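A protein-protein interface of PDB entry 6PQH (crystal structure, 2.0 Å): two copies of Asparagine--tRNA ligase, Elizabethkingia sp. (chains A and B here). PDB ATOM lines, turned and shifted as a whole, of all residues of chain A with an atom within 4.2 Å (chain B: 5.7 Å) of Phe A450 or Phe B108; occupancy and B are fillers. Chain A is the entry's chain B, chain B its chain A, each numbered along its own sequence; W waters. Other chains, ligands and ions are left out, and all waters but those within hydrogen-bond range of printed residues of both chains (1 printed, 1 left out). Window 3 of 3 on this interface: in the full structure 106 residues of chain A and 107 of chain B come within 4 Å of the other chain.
No position is printed for both chains.
Of the 19 pairs that touch across the chains among the printed residues, none has its exchanged pair printed and touching as well.
The indole nitrogen (NE1) of Trp B34 sits at hydrogen-bond distance from the backbone carbonyl oxygen (O) of Gly A451 (2.9 Å).
The backbone NH of Gly A451 sits at hydrogen-bond distance from the backbone carbonyl oxygen of Asp B106, at 2.8 Å.
N of Ser A452 sits at hydrogen-bond distance from O of Asp B106 (3.2 Å).
The backbone NH (N) of Phe B108 lies within hydrogen-bond range of the backbone carbonyl oxygen (O) of Lys A449, at 2.8 Å.
OE2 of Glu B111 is in salt-bridge range of NZ of Lys A449 (3.4 Å).
The guanidinium group (NH1) of Arg B136 sits at hydrogen-bond distance from the backbone carbonyl oxygen (O) of Phe A450 (2.7 Å).
Water W1 lies within hydrogen-bond range of O of Arg A448 (2.7 Å), OD2 of Asp B106 (2.8 Å) and N of Leu A424 (2.9 Å).
Asp B106 touches Lys A449.
Lys A449 touches Asn B107 (O to CA, 3.3 Å).
Ala B75 touches Phe A450 (O to O, 3.6 Å).
O of Phe B108 touches CE1 of Phe A450, 3.5 Å away.
Glu B111 touches Phe A450.
Phe A450 touches Leu B112 (CD1 to CD1, 3.5 Å).
Thr B115 touches Phe A450.
CB of Phe A450 touches CD1 of Leu B117, at 3.8 Å.
O of Ala B75 touches CA of Gly A451, at 3.3 Å.
N of Gly A451 touches CB of Asn B107, at 3.7 Å.
Phe A450 touches just these residues of chain B: Ala B75, Asp B106, Asn B107, Phe B108, Glu B111, Leu B112, Thr B115, Leu B117 and Arg B136.
Phe B108 touches just these residues of chain A: Leu A424, Lys A449 and Phe A450.
Of the printed residues of chain A, Arg B136 touches Phe A450.
Printed residues of chain A within 4 Å of Asp B106: Lys A449 (3.7 Å), Phe A450 (3.8 Å), Gly A451 (2.8 Å) and Ser A452 (3.2 Å).
Asp A446 touches none of the printed residues of chain B.
Glu B110 touches none of the printed residues of chain A.
The nearest residue of chain B that does not touch Phe A450 is Trp B34 (4.5 Å).
O of Ala B75 is in hydrogen-bond range of NH2 of Arg B136, at 3.2 Å.
The side-chain hydroxyl (OG) of Ser B76 is in hydrogen-bond range of the side-chain amide nitrogen (ND2) of Asn B107, at 2.9 Å.
The backbone carbonyl oxygen (O) of Leu B112 lies within hydrogen-bond range of the side-chain hydroxyl (OG1) of Thr B115 (2.9 Å).
The backbone NH (N) of Leu B117 is in hydrogen-bond range of the side-chain hydroxyl (OG1) of Thr B115 (3.0 Å).
OD1 of Asp A446 is in salt-bridge range of NZ of Lys A449 (3.7 Å).
Of the 7 printed residues of chain A, 5 touch a printed residue of chain B.
Hydrophobic or aromatic side chains of chain A that line the printed part of chain B: Leu A424 and Phe A450.
Hydrophobic or aromatic side chains of chain B within 4 Å of the printed part of chain A: Trp B34, Phe B108, Leu B112 and Leu B117.
Among the printed residues, Asp or Glu carboxylates within 4 Å of a Lys or Arg side-chain nitrogen of the other chain: Lys A449 with Glu B111.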
ATOM      1  N   LEU A 424      11.056   1.272   4.156  1.00  0.00           N
ATOM      2  CA  LEU A 424      11.832   1.993   3.148  1.00  0.00           C
ATOM      3  C   LEU A 424      11.479   1.554   1.729  1.00  0.00           C
ATOM      4  O   LEU A 424      11.287   2.393   0.843  1.00  0.00           O
ATOM      5  CB  LEU A 424      13.330   1.803   3.407  1.00  0.00           C
ATOM      6  CG  LEU A 424      14.257   2.392   2.346  1.00  0.00           C
ATOM      7  CD1 LEU A 424      14.234   3.924   2.399  1.00  0.00           C
ATOM      8  CD2 LEU A 424      15.674   1.842   2.492  1.00  0.00           C
ATOM      9  N   ASP A 446      16.469   8.681   5.061  1.00  0.00           N
ATOM     10  CA  ASP A 446      17.325   8.252   6.167  1.00  0.00           C
ATOM     11  C   ASP A 446      16.516   7.862   7.395  1.00  0.00           C
ATOM     12  O   ASP A 446      16.908   6.947   8.128  1.00  0.00           O
ATOM     13  CB  ASP A 446      18.336   9.348   6.526  1.00  0.00           C
ATOM     14  CG  ASP A 446      19.502   9.420   5.538  1.00  0.00           C
ATOM     15  OD1 ASP A 446      19.594   8.542   4.641  1.00  0.00           O
ATOM     16  OD2 ASP A 446      20.325  10.355   5.665  1.00  0.00           O
ATOM     17  N   ARG A 448      14.053   6.112   7.619  1.00  0.00           N
ATOM     18  CA  ARG A 448      13.592   4.739   7.500  1.00  0.00           C
ATOM     19  C   ARG A 448      14.732   3.736   7.487  1.00  0.00           C
ATOM     20  O   ARG A 448      14.489   2.549   7.265  1.00  0.00           O
ATOM     21  CB  ARG A 448      12.762   4.565   6.226  1.00  0.00           C
ATOM     22  CG  ARG A 448      11.270   4.832   6.372  1.00  0.00           C
ATOM     23  CD  ARG A 448      10.992   6.249   6.779  1.00  0.00           C
ATOM     24  NE  ARG A 448       9.584   6.596   6.632  1.00  0.00           N
ATOM     25  CZ  ARG A 448       9.073   7.758   7.019  1.00  0.00           C
ATOM     26  NH1 ARG A 448       9.852   8.675   7.580  1.00  0.00           N
ATOM     27  NH2 ARG A 448       7.783   8.004   6.849  1.00  0.00           N
ATOM     28  N   LYS A 449      15.973   4.181   7.696  1.00  0.00           N
ATOM     29  CA  LYS A 449      17.119   3.307   7.491  1.00  0.00           C
ATOM     30  C   LYS A 449      17.742   2.803   8.782  1.00  0.00           C
ATOM     31  O   LYS A 449      18.419   1.770   8.759  1.00  0.00           O
ATOM     32  CB  LYS A 449      18.209   4.028   6.686  1.00  0.00           C
ATOM     33  CG  LYS A 449      17.864   4.308   5.230  1.00  0.00           C
ATOM     34  CD  LYS A 449      19.015   5.046   4.571  1.00  0.00           C
ATOM     35  CE  LYS A 449      18.920   5.037   3.060  1.00  0.00           C
ATOM     36  NZ  LYS A 449      20.132   5.664   2.454  1.00  0.00           N
ATOM     37  N   PHE A 450      17.557   3.516   9.893  1.00  0.00           N
ATOM     38  CA  PHE A 450      18.307   3.267  11.119  1.00  0.00           C
ATOM     39  C   PHE A 450      17.321   3.176  12.277  1.00  0.00           C
ATOM     40  O   PHE A 450      17.073   4.161  12.978  1.00  0.00           O
ATOM     41  CB  PHE A 450      19.339   4.361  11.322  1.00  0.00           C
ATOM     42  CG  PHE A 450      20.225   4.568  10.130  1.00  0.00           C
ATOM     43  CD1 PHE A 450      21.053   3.546   9.683  1.00  0.00           C
ATOM     44  CD2 PHE A 450      20.230   5.767   9.454  1.00  0.00           C
ATOM     45  CE1 PHE A 450      21.874   3.728   8.581  1.00  0.00           C
ATOM     46  CE2 PHE A 450      21.043   5.950   8.345  1.00  0.00           C
ATOM     47  CZ  PHE A 450      21.862   4.933   7.912  1.00  0.00           C
ATOM     48  N   GLY A 451      16.772   1.986  12.488  1.00  0.00           N
ATOM     49  CA  GLY A 451      15.774   1.852  13.530  1.00  0.00           C
ATOM     50  C   GLY A 451      14.466   2.530  13.184  1.00  0.00           C
ATOM     51  O   GLY A 451      13.881   3.214  14.033  1.00  0.00           O
ATOM     52  N   SER A 452      13.997   2.353  11.953  1.00  0.00           N
ATOM     53  CA  SER A 452      12.699   2.866  11.547  1.00  0.00           C
ATOM     54  C   SER A 452      11.625   2.367  12.507  1.00  0.00           C
ATOM     55  O   SER A 452      11.717   1.257  13.040  1.00  0.00           O
ATOM     56  CB  SER A 452      12.393   2.407  10.117  1.00  0.00           C
ATOM     57  OG  SER A 452      11.227   3.033   9.609  1.00  0.00           O
ATOM     58  N   TRP B  34      14.989   3.309  21.198  1.00  0.00           N
ATOM     59  CA  TRP B  34      16.128   2.986  20.350  1.00  0.00           C
ATOM     60  C   TRP B  34      17.325   2.587  21.200  1.00  0.00           C
ATOM     61  O   TRP B  34      17.512   3.085  22.316  1.00  0.00           O
ATOM     62  CB  TRP B  34      16.518   4.172  19.467  1.00  0.00           C
ATOM     63  CG  TRP B  34      15.459   4.507  18.450  1.00  0.00           C
ATOM     64  CD1 TRP B  34      15.379   4.049  17.169  1.00  0.00           C
ATOM     65  CD2 TRP B  34      14.325   5.352  18.646  1.00  0.00           C
ATOM     66  NE1 TRP B  34      14.266   4.571  16.548  1.00  0.00           N
ATOM     67  CE2 TRP B  34      13.599   5.369  17.440  1.00  0.00           C
ATOM     68  CE3 TRP B  34      13.856   6.106  19.724  1.00  0.00           C
ATOM     69  CZ2 TRP B  34      12.434   6.116  17.277  1.00  0.00           C
ATOM     70  CZ3 TRP B  34      12.692   6.843  19.562  1.00  0.00           C
ATOM     71  CH2 TRP B  34      11.999   6.845  18.346  1.00  0.00           C
ATOM     72  N   ALA B  75      21.228   1.871  17.488  1.00  0.00           N
ATOM     73  CA  ALA B  75      20.173   2.634  16.837  1.00  0.00           C
ATOM     74  C   ALA B  75      18.993   1.763  16.404  1.00  0.00           C
ATOM     75  O   ALA B  75      18.007   2.315  15.902  1.00  0.00           O
ATOM     76  CB  ALA B  75      20.683   3.450  15.634  1.00  0.00           C
ATOM     77  N   SER B  76      19.029   0.445  16.609  1.00  0.00           N
ATOM     78  CA  SER B  76      17.843  -0.361  16.338  1.00  0.00           C
ATOM     79  C   SER B  76      16.669   0.090  17.197  1.00  0.00           C
ATOM     80  O   SER B  76      16.830   0.577  18.319  1.00  0.00           O
ATOM     81  CB  SER B  76      18.110  -1.844  16.603  1.00  0.00           C
ATOM     82  OG  SER B  76      19.184  -2.310  15.815  1.00  0.00           O
ATOM     83  N   ASP B 106      13.714  -1.580  10.051  1.00  0.00           N
ATOM     84  CA  ASP B 106      15.027  -1.816   9.456  1.00  0.00           C
ATOM     85  C   ASP B 106      16.107  -1.051  10.210  1.00  0.00           C
ATOM     86  O   ASP B 106      15.870   0.038  10.736  1.00  0.00           O
ATOM     87  CB  ASP B 106      15.067  -1.361   7.991  1.00  0.00           C
ATOM     88  CG  ASP B 106      14.257  -2.252   7.055  1.00  0.00           C
ATOM     89  OD1 ASP B 106      14.135  -3.461   7.308  1.00  0.00           O
ATOM     90  OD2 ASP B 106      13.761  -1.735   6.037  1.00  0.00           O
ATOM     91  N   ASN B 107      17.314  -1.620  10.232  1.00  0.00           N
ATOM     92  CA  ASN B 107      18.508  -0.891  10.653  1.00  0.00           C
ATOM     93  C   ASN B 107      19.658  -1.337   9.757  1.00  0.00           C
ATOM     94  O   ASN B 107      20.179  -2.448   9.911  1.00  0.00           O
ATOM     95  CB  ASN B 107      18.820  -1.131  12.130  1.00  0.00           C
ATOM     96  CG  ASN B 107      19.955  -0.257  12.632  1.00  0.00           C
ATOM     97  OD1 ASN B 107      20.413   0.649  11.938  1.00  0.00           O
ATOM     98  ND2 ASN B 107      20.414  -0.530  13.844  1.00  0.00           N
ATOM     99  N   PHE B 108      20.045  -0.491   8.806  1.00  0.00           N
ATOM    100  CA  PHE B 108      21.086  -0.876   7.855  1.00  0.00           C
ATOM    101  C   PHE B 108      22.436  -0.603   8.500  1.00  0.00           C
ATOM    102  O   PHE B 108      23.044   0.455   8.328  1.00  0.00           O
ATOM    103  CB  PHE B 108      20.885  -0.153   6.535  1.00  0.00           C
ATOM    104  CG  PHE B 108      19.631  -0.588   5.819  1.00  0.00           C
ATOM    105  CD1 PHE B 108      19.625  -1.728   5.033  1.00  0.00           C
ATOM    106  CD2 PHE B 108      18.445   0.115   5.971  1.00  0.00           C
ATOM    107  CE1 PHE B 108      18.469  -2.140   4.390  1.00  0.00           C
ATOM    108  CE2 PHE B 108      17.288  -0.294   5.329  1.00  0.00           C
ATOM    109  CZ  PHE B 108      17.297  -1.420   4.543  1.00  0.00           C
ATOM    110  N   THR B 109      22.903  -1.601   9.263  1.00  0.00           N
ATOM    111  CA  THR B 109      24.054  -1.411  10.137  1.00  0.00           C
ATOM    112  C   THR B 109      25.325  -1.098   9.355  1.00  0.00           C
ATOM    113  O   THR B 109      26.217  -0.419   9.877  1.00  0.00           O
ATOM    114  CB  THR B 109      24.247  -2.650  11.013  1.00  0.00           C
ATOM    115  OG1 THR B 109      24.345  -3.814  10.185  1.00  0.00           O
ATOM    116  CG2 THR B 109      23.057  -2.811  11.953  1.00  0.00           C
ATOM    117  N   GLU B 110      25.418  -1.552   8.100  1.00  0.00           N
ATOM    118  CA  GLU B 110      26.591  -1.252   7.285  1.00  0.00           C
ATOM    119  C   GLU B 110      26.724   0.245   7.036  1.00  0.00           C
ATOM    120  O   GLU B 110      27.838   0.780   7.006  1.00  0.00           O
ATOM    121  CB  GLU B 110      26.526  -2.002   5.951  1.00  0.00           C
ATOM    122  CG  GLU B 110      25.596  -3.216   5.916  1.00  0.00           C
ATOM    123  CD  GLU B 110      24.125  -2.839   5.776  1.00  0.00           C
ATOM    124  OE1 GLU B 110      23.349  -3.129   6.712  1.00  0.00           O
ATOM    125  OE2 GLU B 110      23.750  -2.249   4.737  1.00  0.00           O
ATOM    126  N   GLU B 111      25.593   0.940   6.862  1.00  0.00           N
ATOM    127  CA  GLU B 111      25.583   2.370   6.577  1.00  0.00           C
ATOM    128  C   GLU B 111      25.668   3.227   7.834  1.00  0.00           C
ATOM    129  O   GLU B 111      25.894   4.436   7.731  1.00  0.00           O
ATOM    130  CB  GLU B 111      24.316   2.733   5.789  1.00  0.00           C
ATOM    131  CG  GLU B 111      24.228   2.108   4.397  1.00  0.00           C
ATOM    132  CD  GLU B 111      23.001   2.567   3.616  1.00  0.00           C
ATOM    133  OE1 GLU B 111      22.281   1.704   3.064  1.00  0.00           O
ATOM    134  OE2 GLU B 111      22.757   3.793   3.561  1.00  0.00           O
ATOM    135  N   LEU B 112      25.492   2.630   9.010  1.00  0.00           N
ATOM    136  CA  LEU B 112      25.525   3.393  10.251  1.00  0.00           C
ATOM    137  C   LEU B 112      26.874   4.066  10.453  1.00  0.00           C
ATOM    138  O   LEU B 112      26.946   5.144  11.054  1.00  0.00           O
ATOM    139  CB  LEU B 112      25.205   2.466  11.421  1.00  0.00           C
ATOM    140  CG  LEU B 112      24.660   3.090  12.693  1.00  0.00           C
ATOM    141  CD1 LEU B 112      23.296   3.688  12.428  1.00  0.00           C
ATOM    142  CD2 LEU B 112      24.577   2.025  13.761  1.00  0.00           C
ATOM    143  N   THR B 115      27.113   7.723   9.509  1.00  0.00           N
ATOM    144  CA  THR B 115      26.221   8.651  10.182  1.00  0.00           C
ATOM    145  C   THR B 115      26.770   9.041  11.547  1.00  0.00           C
ATOM    146  O   THR B 115      27.711   8.437  12.070  1.00  0.00           O
ATOM    147  CB  THR B 115      24.828   8.045  10.365  1.00  0.00           C
ATOM    148  OG1 THR B 115      24.857   7.148  11.484  1.00  0.00           O
ATOM    149  CG2 THR B 115      24.410   7.282   9.109  1.00  0.00           C
ATOM    150  N   LEU B 117      25.153   8.520  14.134  1.00  0.00           N
ATOM    151  CA  LEU B 117      24.609   7.555  15.078  1.00  0.00           C
ATOM    152  C   LEU B 117      25.657   6.563  15.545  1.00  0.00           C
ATOM    153  O   LEU B 117      25.434   5.867  16.544  1.00  0.00           O
ATOM    154  CB  LEU B 117      23.431   6.801  14.460  1.00  0.00           C
ATOM    155  CG  LEU B 117      22.268   7.717  14.067  1.00  0.00           C
ATOM    156  CD1 LEU B 117      21.185   6.942  13.348  1.00  0.00           C
ATOM    157  CD2 LEU B 117      21.702   8.444  15.281  1.00  0.00           C
ATOM    158  N   LEU B 133      19.505  13.912  11.706  1.00  0.00           N
ATOM    159  CA  LEU B 133      19.804  12.809  12.611  1.00  0.00           C
ATOM    160  C   LEU B 133      20.272  13.249  13.991  1.00  0.00           C
ATOM    161  O   LEU B 133      20.235  12.439  14.927  1.00  0.00           O
ATOM    162  CB  LEU B 133      20.877  11.904  11.998  1.00  0.00           C
ATOM    163  CG  LEU B 133      20.492  11.171  10.716  1.00  0.00           C
ATOM    164  CD1 LEU B 133      21.643  10.288  10.241  1.00  0.00           C
ATOM    165  CD2 LEU B 133      19.231  10.342  10.972  1.00  0.00           C
ATOM    166  N   ARG B 136      18.841  12.508  17.641  1.00  0.00           N
ATOM    167  CA  ARG B 136      18.994  11.197  18.252  1.00  0.00           C
ATOM    168  C   ARG B 136      20.258  11.081  19.094  1.00  0.00           C
ATOM    169  O   ARG B 136      20.601   9.979  19.519  1.00  0.00           O
ATOM    170  CB  ARG B 136      18.974  10.123  17.157  1.00  0.00           C
ATOM    171  CG  ARG B 136      17.663  10.156  16.343  1.00  0.00           C
ATOM    172  CD  ARG B 136      17.656   9.149  15.168  1.00  0.00           C
ATOM    173  NE  ARG B 136      17.848   7.772  15.607  1.00  0.00           N
ATOM    174  CZ  ARG B 136      17.620   6.702  14.857  1.00  0.00           C
ATOM    175  NH1 ARG B 136      17.164   6.834  13.610  1.00  0.00           N
ATOM    176  NH2 ARG B 136      17.845   5.494  15.363  1.00  0.00           N
HETATM  177  O   HOH W   1      12.524   0.740   6.656  1.00  0.00           O
